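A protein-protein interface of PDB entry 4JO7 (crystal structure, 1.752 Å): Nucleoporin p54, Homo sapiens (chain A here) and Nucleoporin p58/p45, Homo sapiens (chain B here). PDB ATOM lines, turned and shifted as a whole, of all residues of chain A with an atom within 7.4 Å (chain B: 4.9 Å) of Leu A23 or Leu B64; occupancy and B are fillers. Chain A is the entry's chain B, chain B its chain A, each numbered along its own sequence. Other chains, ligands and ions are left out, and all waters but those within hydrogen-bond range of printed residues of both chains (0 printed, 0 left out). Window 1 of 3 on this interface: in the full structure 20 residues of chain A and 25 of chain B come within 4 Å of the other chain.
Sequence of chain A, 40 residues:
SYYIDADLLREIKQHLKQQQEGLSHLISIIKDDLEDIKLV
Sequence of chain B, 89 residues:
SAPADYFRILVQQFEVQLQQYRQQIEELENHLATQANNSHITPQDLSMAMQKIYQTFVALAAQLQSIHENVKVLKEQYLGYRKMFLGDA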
ATOM      1  N   LYS A  17     -19.757  19.574  -5.281  1.00  0.00           N
ATOM      2  CA  LYS A  17     -18.910  18.554  -4.674  1.00  0.00           C
ATOM      3  C   LYS A  17     -18.846  18.711  -3.152  1.00  0.00           C
ATOM      4  O   LYS A  17     -18.930  17.736  -2.404  1.00  0.00           O
ATOM      5  CB  LYS A  17     -17.503  18.633  -5.270  1.00  0.00           C
ATOM      6  CG  LYS A  17     -16.500  17.663  -4.657  1.00  0.00           C
ATOM      7  CD  LYS A  17     -16.882  16.213  -4.911  1.00  0.00           C
ATOM      8  CE  LYS A  17     -15.836  15.264  -4.332  1.00  0.00           C
ATOM      9  NZ  LYS A  17     -16.278  13.844  -4.387  1.00  0.00           N
ATOM     10  N   GLN A  18     -18.705  19.943  -2.691  1.00  0.00           N
ATOM     11  CA  GLN A  18     -18.661  20.188  -1.259  1.00  0.00           C
ATOM     12  C   GLN A  18     -19.980  19.767  -0.598  1.00  0.00           C
ATOM     13  O   GLN A  18     -19.984  19.277   0.531  1.00  0.00           O
ATOM     14  CB  GLN A  18     -18.354  21.655  -0.975  1.00  0.00           C
ATOM     15  CG  GLN A  18     -18.072  21.948   0.488  1.00  0.00           C
ATOM     16  CD  GLN A  18     -17.366  23.277   0.690  1.00  0.00           C
ATOM     17  OE1 GLN A  18     -17.036  23.969  -0.271  1.00  0.00           O
ATOM     18  NE2 GLN A  18     -17.129  23.635   1.946  1.00  0.00           N
ATOM     19  N   GLN A  19     -21.098  19.952  -1.295  1.00  0.00           N
ATOM     20  CA  GLN A  19     -22.393  19.523  -0.757  1.00  0.00           C
ATOM     21  C   GLN A  19     -22.511  18.005  -0.738  1.00  0.00           C
ATOM     22  O   GLN A  19     -23.075  17.425   0.197  1.00  0.00           O
ATOM     23  CB  GLN A  19     -23.538  20.124  -1.570  1.00  0.00           C
ATOM     24  CG  GLN A  19     -23.516  21.630  -1.582  1.00  0.00           C
ATOM     25  CD  GLN A  19     -24.572  22.214  -2.478  1.00  0.00           C
ATOM     26  OE1 GLN A  19     -25.246  21.506  -3.240  1.00  0.00           O
ATOM     27  NE2 GLN A  19     -24.739  23.513  -2.386  1.00  0.00           N
ATOM     28  N   GLN A  20     -21.990  17.353  -1.769  1.00  0.00           N
ATOM     29  CA  GLN A  20     -21.940  15.898  -1.781  1.00  0.00           C
ATOM     30  C   GLN A  20     -21.156  15.385  -0.577  1.00  0.00           C
ATOM     31  O   GLN A  20     -21.545  14.405   0.057  1.00  0.00           O
ATOM     32  CB  GLN A  20     -21.290  15.391  -3.067  1.00  0.00           C
ATOM     33  CG  GLN A  20     -22.117  15.652  -4.317  1.00  0.00           C
ATOM     34  CD  GLN A  20     -21.305  15.512  -5.589  1.00  0.00           C
ATOM     35  OE1 GLN A  20     -21.400  16.347  -6.486  1.00  0.00           O
ATOM     36  NE2 GLN A  20     -20.491  14.461  -5.666  1.00  0.00           N
ATOM     37  N   GLU A  21     -20.038  16.039  -0.280  1.00  0.00           N
ATOM     38  CA  GLU A  21     -19.198  15.647   0.852  1.00  0.00           C
ATOM     39  C   GLU A  21     -19.925  15.836   2.182  1.00  0.00           C
ATOM     40  O   GLU A  21     -19.724  15.065   3.121  1.00  0.00           O
ATOM     41  CB  GLU A  21     -17.886  16.435   0.842  1.00  0.00           C
ATOM     42  CG  GLU A  21     -16.958  16.058  -0.298  1.00  0.00           C
ATOM     43  CD  GLU A  21     -15.784  17.009  -0.445  1.00  0.00           C
ATOM     44  OE1 GLU A  21     -15.751  18.042   0.259  1.00  0.00           O
ATOM     45  OE2 GLU A  21     -14.889  16.716  -1.265  1.00  0.00           O
ATOM     46  N   GLY A  22     -20.754  16.840   2.277  1.00  0.00           N
ATOM     47  CA  GLY A  22     -21.548  17.072   3.449  1.00  0.00           C
ATOM     48  C   GLY A  22     -22.516  15.920   3.755  1.00  0.00           C
ATOM     49  O   GLY A  22     -22.669  15.485   4.852  1.00  0.00           O
ATOM     50  N   LEU A  23     -23.178  15.472   2.707  1.00  0.00           N
ATOM     51  CA  LEU A  23     -24.081  14.355   2.818  1.00  0.00           C
ATOM     52  C   LEU A  23     -23.272  13.136   3.204  1.00  0.00           C
ATOM     53  O   LEU A  23     -23.636  12.413   4.027  1.00  0.00           O
ATOM     54  CB  LEU A  23     -24.807  14.087   1.504  1.00  0.00           C
ATOM     55  CG  LEU A  23     -25.775  15.161   1.043  1.00  0.00           C
ATOM     56  CD1 LEU A  23     -26.415  14.872  -0.278  1.00  0.00           C
ATOM     57  CD2 LEU A  23     -26.827  15.465   2.052  1.00  0.00           C
ATOM     58  N   SER A  24     -22.154  12.971   2.522  1.00  0.00           N
ATOM     59  CA  SER A  24     -21.284  11.805   2.924  1.00  0.00           C
ATOM     60  C   SER A  24     -20.768  11.691   4.464  1.00  0.00           C
ATOM     61  O   SER A  24     -20.889  10.714   5.059  1.00  0.00           O
ATOM     62  CB  SER A  24     -20.059  11.760   2.013  1.00  0.00           C
ATOM     63  OG  SER A  24     -20.445  11.466   0.681  1.00  0.00           O
ATOM     64  N   HIS A  25     -20.561  12.877   5.017  1.00  0.00           N
ATOM     65  CA  HIS A  25     -20.266  13.006   6.430  1.00  0.00           C
ATOM     66  C   HIS A  25     -21.442  12.597   7.293  1.00  0.00           C
ATOM     67  O   HIS A  25     -21.261  12.029   8.314  1.00  0.00           O
ATOM     68  CB  HIS A  25     -19.797  14.406   6.791  1.00  0.00           C
ATOM     69  CG  HIS A  25     -18.973  14.470   8.050  1.00  0.00           C
ATOM     70  ND1 HIS A  25     -18.829  13.426   8.899  1.00  0.00           N
ATOM     71  CD2 HIS A  25     -18.237  15.506   8.597  1.00  0.00           C
ATOM     72  CE1 HIS A  25     -18.039  13.786   9.893  1.00  0.00           C
ATOM     73  NE2 HIS A  25     -17.671  15.052   9.703  1.00  0.00           N
ATOM     74  N   LEU A  26     -22.653  12.880   6.860  1.00  0.00           N
ATOM     75  CA  LEU A  26     -23.830  12.456   7.616  1.00  0.00           C
ATOM     76  C   LEU A  26     -23.911  10.930   7.625  1.00  0.00           C
ATOM     77  O   LEU A  26     -24.199  10.355   8.560  1.00  0.00           O
ATOM     78  CB  LEU A  26     -25.110  13.031   7.098  1.00  0.00           C
ATOM     79  CG  LEU A  26     -25.260  14.550   7.114  1.00  0.00           C
ATOM     80  CD1 LEU A  26     -26.576  14.991   6.513  1.00  0.00           C
ATOM     81  CD2 LEU A  26     -25.056  15.140   8.502  1.00  0.00           C
ATOM     82  N   ILE A  27     -23.655  10.344   6.475  1.00  0.00           N
ATOM     83  CA  ILE A  27     -23.690   8.913   6.338  1.00  0.00           C
ATOM     84  C   ILE A  27     -22.679   8.246   7.257  1.00  0.00           C
ATOM     85  O   ILE A  27     -22.952   7.276   7.857  1.00  0.00           O
ATOM     86  CB  ILE A  27     -23.507   8.481   4.871  1.00  0.00           C
ATOM     87  CG1 ILE A  27     -24.723   8.908   4.081  1.00  0.00           C
ATOM     88  CG2 ILE A  27     -23.293   6.999   4.769  1.00  0.00           C
ATOM     89  CD1 ILE A  27     -24.633   8.734   2.604  1.00  0.00           C
ATOM     90  N   SER A  28     -21.492   8.811   7.314  1.00  0.00           N
ATOM     91  CA  SER A  28     -20.465   8.287   8.191  1.00  0.00           C
ATOM     92  C   SER A  28     -20.957   8.165   9.624  1.00  0.00           C
ATOM     93  O   SER A  28     -20.659   7.239  10.276  1.00  0.00           O
ATOM     94  CB  SER A  28     -19.168   9.119   8.173  1.00  0.00           C
ATOM     95  OG  SER A  28     -18.556   8.989   6.967  1.00  0.00           O
ATOM     96  N   ILE A  29     -21.681   9.147  10.083  1.00  0.00           N
ATOM     97  CA  ILE A  29     -22.152   9.133  11.465  1.00  0.00           C
ATOM     98  C   ILE A  29     -23.192   8.028  11.632  1.00  0.00           C
ATOM     99  O   ILE A  29     -23.176   7.314  12.624  1.00  0.00           O
ATOM    100  CB  ILE A  29     -22.726  10.495  11.898  1.00  0.00           C
ATOM    101  CG1 ILE A  29     -21.614  11.545  11.916  1.00  0.00           C
ATOM    102  CG2 ILE A  29     -23.376  10.395  13.295  1.00  0.00           C
ATOM    103  CD1 ILE A  29     -22.096  12.937  12.252  1.00  0.00           C
ATOM    104  N   ILE A  30     -24.072   7.873  10.645  1.00  0.00           N
ATOM    105  CA  ILE A  30     -25.068   6.802  10.670  1.00  0.00           C
ATOM    106  C   ILE A  30     -24.402   5.423  10.691  1.00  0.00           C
ATOM    107  O   ILE A  30     -24.844   4.516  11.399  1.00  0.00           O
ATOM    108  CB  ILE A  30     -26.035   6.908   9.469  1.00  0.00           C
ATOM    109  CG1 ILE A  30     -26.920   8.147   9.612  1.00  0.00           C
ATOM    110  CG2 ILE A  30     -26.897   5.654   9.356  1.00  0.00           C
ATOM    111  CD1 ILE A  30     -27.530   8.620   8.299  1.00  0.00           C
ATOM    112  N   PHE B   7     -24.133  15.529  14.532  1.00  0.00           N
ATOM    113  CA  PHE B   7     -25.002  15.320  13.369  1.00  0.00           C
ATOM    114  C   PHE B   7     -25.944  16.514  13.195  1.00  0.00           C
ATOM    115  O   PHE B   7     -26.108  17.043  12.092  1.00  0.00           O
ATOM    116  CB  PHE B   7     -25.793  14.006  13.528  1.00  0.00           C
ATOM    117  CG  PHE B   7     -26.563  13.594  12.293  1.00  0.00           C
ATOM    118  CD1 PHE B   7     -27.795  14.160  12.007  1.00  0.00           C
ATOM    119  CD2 PHE B   7     -26.066  12.625  11.443  1.00  0.00           C
ATOM    120  CE1 PHE B   7     -28.509  13.784  10.883  1.00  0.00           C
ATOM    121  CE2 PHE B   7     -26.778  12.236  10.312  1.00  0.00           C
ATOM    122  CZ  PHE B   7     -28.001  12.821  10.032  1.00  0.00           C
ATOM    123  N   PHE B  14     -25.152  22.462   6.920  1.00  0.00           N
ATOM    124  CA  PHE B  14     -25.438  22.062   5.547  1.00  0.00           C
ATOM    125  C   PHE B  14     -26.510  22.962   4.946  1.00  0.00           C
ATOM    126  O   PHE B  14     -26.383  23.423   3.815  1.00  0.00           O
ATOM    127  CB  PHE B  14     -25.900  20.603   5.510  1.00  0.00           C
ATOM    128  CG  PHE B  14     -26.080  20.060   4.122  1.00  0.00           C
ATOM    129  CD1 PHE B  14     -24.990  19.640   3.386  1.00  0.00           C
ATOM    130  CD2 PHE B  14     -27.339  19.971   3.556  1.00  0.00           C
ATOM    131  CE1 PHE B  14     -25.151  19.139   2.108  1.00  0.00           C
ATOM    132  CE2 PHE B  14     -27.503  19.469   2.281  1.00  0.00           C
ATOM    133  CZ  PHE B  14     -26.410  19.051   1.561  1.00  0.00           C
ATOM    134  N   PHE B  57     -30.718  18.013  -3.394  1.00  0.00           N
ATOM    135  CA  PHE B  57     -29.826  18.054  -2.241  1.00  0.00           C
ATOM    136  C   PHE B  57     -30.605  18.255  -0.941  1.00  0.00           C
ATOM    137  O   PHE B  57     -30.289  17.641   0.076  1.00  0.00           O
ATOM    138  CB  PHE B  57     -28.772  19.161  -2.390  1.00  0.00           C
ATOM    139  CG  PHE B  57     -27.554  18.734  -3.159  1.00  0.00           C
ATOM    140  CD1 PHE B  57     -26.608  17.911  -2.574  1.00  0.00           C
ATOM    141  CD2 PHE B  57     -27.359  19.151  -4.468  1.00  0.00           C
ATOM    142  CE1 PHE B  57     -25.478  17.513  -3.275  1.00  0.00           C
ATOM    143  CE2 PHE B  57     -26.233  18.756  -5.175  1.00  0.00           C
ATOM    144  CZ  PHE B  57     -25.294  17.938  -4.581  1.00  0.00           C
ATOM    145  N   LEU B  60     -32.280  14.986  -0.094  1.00  0.00           N
ATOM    146  CA  LEU B  60     -31.339  13.979   0.388  1.00  0.00           C
ATOM    147  C   LEU B  60     -30.948  14.229   1.841  1.00  0.00           C
ATOM    148  O   LEU B  60     -30.860  13.291   2.630  1.00  0.00           O
ATOM    149  CB  LEU B  60     -30.082  13.941  -0.487  1.00  0.00           C
ATOM    150  CG  LEU B  60     -30.262  13.259  -1.843  1.00  0.00           C
ATOM    151  CD1 LEU B  60     -29.123  13.619  -2.793  1.00  0.00           C
ATOM    152  CD2 LEU B  60     -30.361  11.754  -1.653  1.00  0.00           C
ATOM    153  N   ALA B  61     -30.727  15.488   2.202  1.00  0.00           N
ATOM    154  CA  ALA B  61     -30.358  15.815   3.570  1.00  0.00           C
ATOM    155  C   ALA B  61     -31.488  15.440   4.521  1.00  0.00           C
ATOM    156  O   ALA B  61     -31.247  14.877   5.587  1.00  0.00           O
ATOM    157  CB  ALA B  61     -30.012  17.298   3.710  1.00  0.00           C
ATOM    158  N   ALA B  62     -32.721  15.757   4.140  1.00  0.00           N
ATOM    159  CA  ALA B  62     -33.874  15.406   4.959  1.00  0.00           C
ATOM    160  C   ALA B  62     -34.032  13.899   5.081  1.00  0.00           C
ATOM    161  O   ALA B  62     -34.368  13.390   6.154  1.00  0.00           O
ATOM    162  CB  ALA B  62     -35.141  16.042   4.405  1.00  0.00           C
ATOM    163  N   GLN B  63     -33.792  13.171   3.993  1.00  0.00           N
ATOM    164  CA  GLN B  63     -33.917  11.719   4.028  1.00  0.00           C
ATOM    165  C   GLN B  63     -32.872  11.099   4.948  1.00  0.00           C
ATOM    166  O   GLN B  63     -33.156  10.147   5.681  1.00  0.00           O
ATOM    167  CB  GLN B  63     -33.786  11.136   2.622  1.00  0.00           C
ATOM    168  CG  GLN B  63     -34.910  11.515   1.679  1.00  0.00           C
ATOM    169  CD  GLN B  63     -34.739  10.890   0.309  1.00  0.00           C
ATOM    170  OE1 GLN B  63     -33.742  11.134  -0.381  1.00  0.00           O
ATOM    171  NE2 GLN B  63     -35.701  10.070  -0.089  1.00  0.00           N
ATOM    172  N   LEU B  64     -31.656  11.626   4.914  1.00  0.00           N
ATOM    173  CA  LEU B  64     -30.605  11.098   5.778  1.00  0.00           C
ATOM    174  C   LEU B  64     -30.890  11.432   7.249  1.00  0.00           C
ATOM    175  O   LEU B  64     -30.623  10.622   8.138  1.00  0.00           O
ATOM    176  CB  LEU B  64     -29.228  11.614   5.339  1.00  0.00           C
ATOM    177  CG  LEU B  64     -28.736  11.003   4.017  1.00  0.00           C
ATOM    178  CD1 LEU B  64     -27.519  11.747   3.493  1.00  0.00           C
ATOM    179  CD2 LEU B  64     -28.421   9.524   4.174  1.00  0.00           C
ATOM    180  N   GLN B  65     -31.459  12.604   7.507  1.00  0.00           N
ATOM    181  CA  GLN B  65     -31.858  12.945   8.869  1.00  0.00           C
ATOM    182  C   GLN B  65     -32.905  11.933   9.368  1.00  0.00           C
ATOM    183  O   GLN B  65     -32.835  11.451  10.505  1.00  0.00           O
ATOM    184  CB  GLN B  65     -32.384  14.384   8.937  1.00  0.00           C
ATOM    185  CG  GLN B  65     -32.615  14.904  10.358  1.00  0.00           C
ATOM    186  CD  GLN B  65     -32.694  16.428  10.427  1.00  0.00           C
ATOM    187  OE1 GLN B  65     -33.273  17.074   9.554  1.00  0.00           O
ATOM    188  NE2 GLN B  65     -32.099  17.005  11.465  1.00  0.00           N
ATOM    189  N   SER B  66     -33.861  11.581   8.514  1.00  0.00           N
ATOM    190  CA  SER B  66     -34.862  10.584   8.886  1.00  0.00           C
ATOM    191  C   SER B  66     -34.250   9.203   9.122  1.00  0.00           C
ATOM    192  O   SER B  66     -34.678   8.487  10.027  1.00  0.00           O
ATOM    193  CB  SER B  66     -35.975  10.503   7.842  1.00  0.00           C
ATOM    194  OG  SER B  66     -36.946  11.501   8.087  1.00  0.00           O
ATOM    195  N   ILE B  67     -33.260   8.818   8.317  1.00  0.00           N
ATOM    196  CA  ILE B  67     -32.562   7.555   8.553  1.00  0.00           C
ATOM    197  C   ILE B  67     -31.944   7.610   9.948  1.00  0.00           C
ATOM    198  O   ILE B  67     -32.074   6.676  10.741  1.00  0.00           O
ATOM    199  CB  ILE B  67     -31.437   7.297   7.518  1.00  0.00           C
ATOM    200  CG1 ILE B  67     -32.022   6.977   6.141  1.00  0.00           C
ATOM    201  CG2 ILE B  67     -30.526   6.171   7.982  1.00  0.00           C
ATOM    202  CD1 ILE B  67     -32.726   5.646   6.058  1.00  0.00           C
ATOM    203  N   HIS B  68     -31.274   8.722  10.250  1.00  0.00           N
ATOM    204  CA  HIS B  68     -30.606   8.878  11.541  1.00  0.00           C
ATOM    205  C   HIS B  68     -31.612   8.721  12.683  1.00  0.00           C
ATOM    206  O   HIS B  68     -31.369   7.989  13.643  1.00  0.00           O
ATOM    207  CB  HIS B  68     -29.923  10.242  11.602  1.00  0.00           C
ATOM    208  CG  HIS B  68     -28.998  10.416  12.767  1.00  0.00           C
ATOM    209  ND1 HIS B  68     -29.149  11.426  13.690  1.00  0.00           N
ATOM    210  CD2 HIS B  68     -27.893   9.728  13.142  1.00  0.00           C
ATOM    211  CE1 HIS B  68     -28.187  11.348  14.592  1.00  0.00           C
ATOM    212  NE2 HIS B  68     -27.413  10.322  14.284  1.00  0.00           N
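Of chain B, only Phe B14 (3.6 Å), Phe B57 (3.8 Å), Leu B60 (3.8 Å), Ala B61 (3.9 Å) and Leu B64 (3.98 Å) come within 4 Å of Leu A23. Of the printed residues of chain B, Ile A27 touches Leu B64 (3.8 Å). Of the printed residues of chain B, Ile A29 touches Phe B7. Leu B64 touches three residues of chain A. Gln B65 touches none of the printed residues of chain A. The nearest printed residue of chain B that does not touch Gln A20 is Phe B14 (5.3 Å).
Of the 14 printed residues of chain A, 7 touch a printed residue of chain B. Printed residues of chain A that touch a printed residue of chain B: Gln A19, Gln A20, Leu A23, Leu A26, Ile A27, Ile A29 and Ile A30. Hydrophobic or aromatic side chains of chain A within 4 Å of the printed part of chain B: Leu A23, Leu A26, Ile A27, Ile A29 and Ile A30. Printed residues of chain B that touch a printed residue of chain A: Phe B7, Phe B14, Phe B57, Leu B60, Ala B61, Leu B64, Ile B67 and His B68. Hydrophobic or aromatic side chains of chain B that line the printed part of chain A: Phe B7, Phe B14, Phe B57, Leu B60, Leu B64, Ile B67 and His B68. Among the printed residues, 14 pairs touch across the chains.
Among the printed residues, pairs that only touch across the chains: Gln A19 with Phe B14 (3.3 Å), Gln A19 with Phe B57 (3.4 Å), Leu A26 with Phe B7 (3.6 Å), Leu A23 with Phe B14 (3.6 Å), Ile A30 with Leu B64 (3.7 Å), Ile A27 with Leu B64 (3.8 Å), Leu A23 with Leu B60 (3.8 Å), Gln A20 with Phe B57 (3.8 Å), Leu A23 with Phe B57 (3.8 Å), Leu A23 with Ala B61 (3.9 Å), Ile A30 with Ile B67 (3.9 Å), Ile A29 with Phe B7 (3.9 Å), Leu A23 with Leu B64 (3.98 Å) and Ile A30 with His B68 (3.99 Å).
OG of Ser A24 is in hydrogen-bond range of O of Gln A20.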
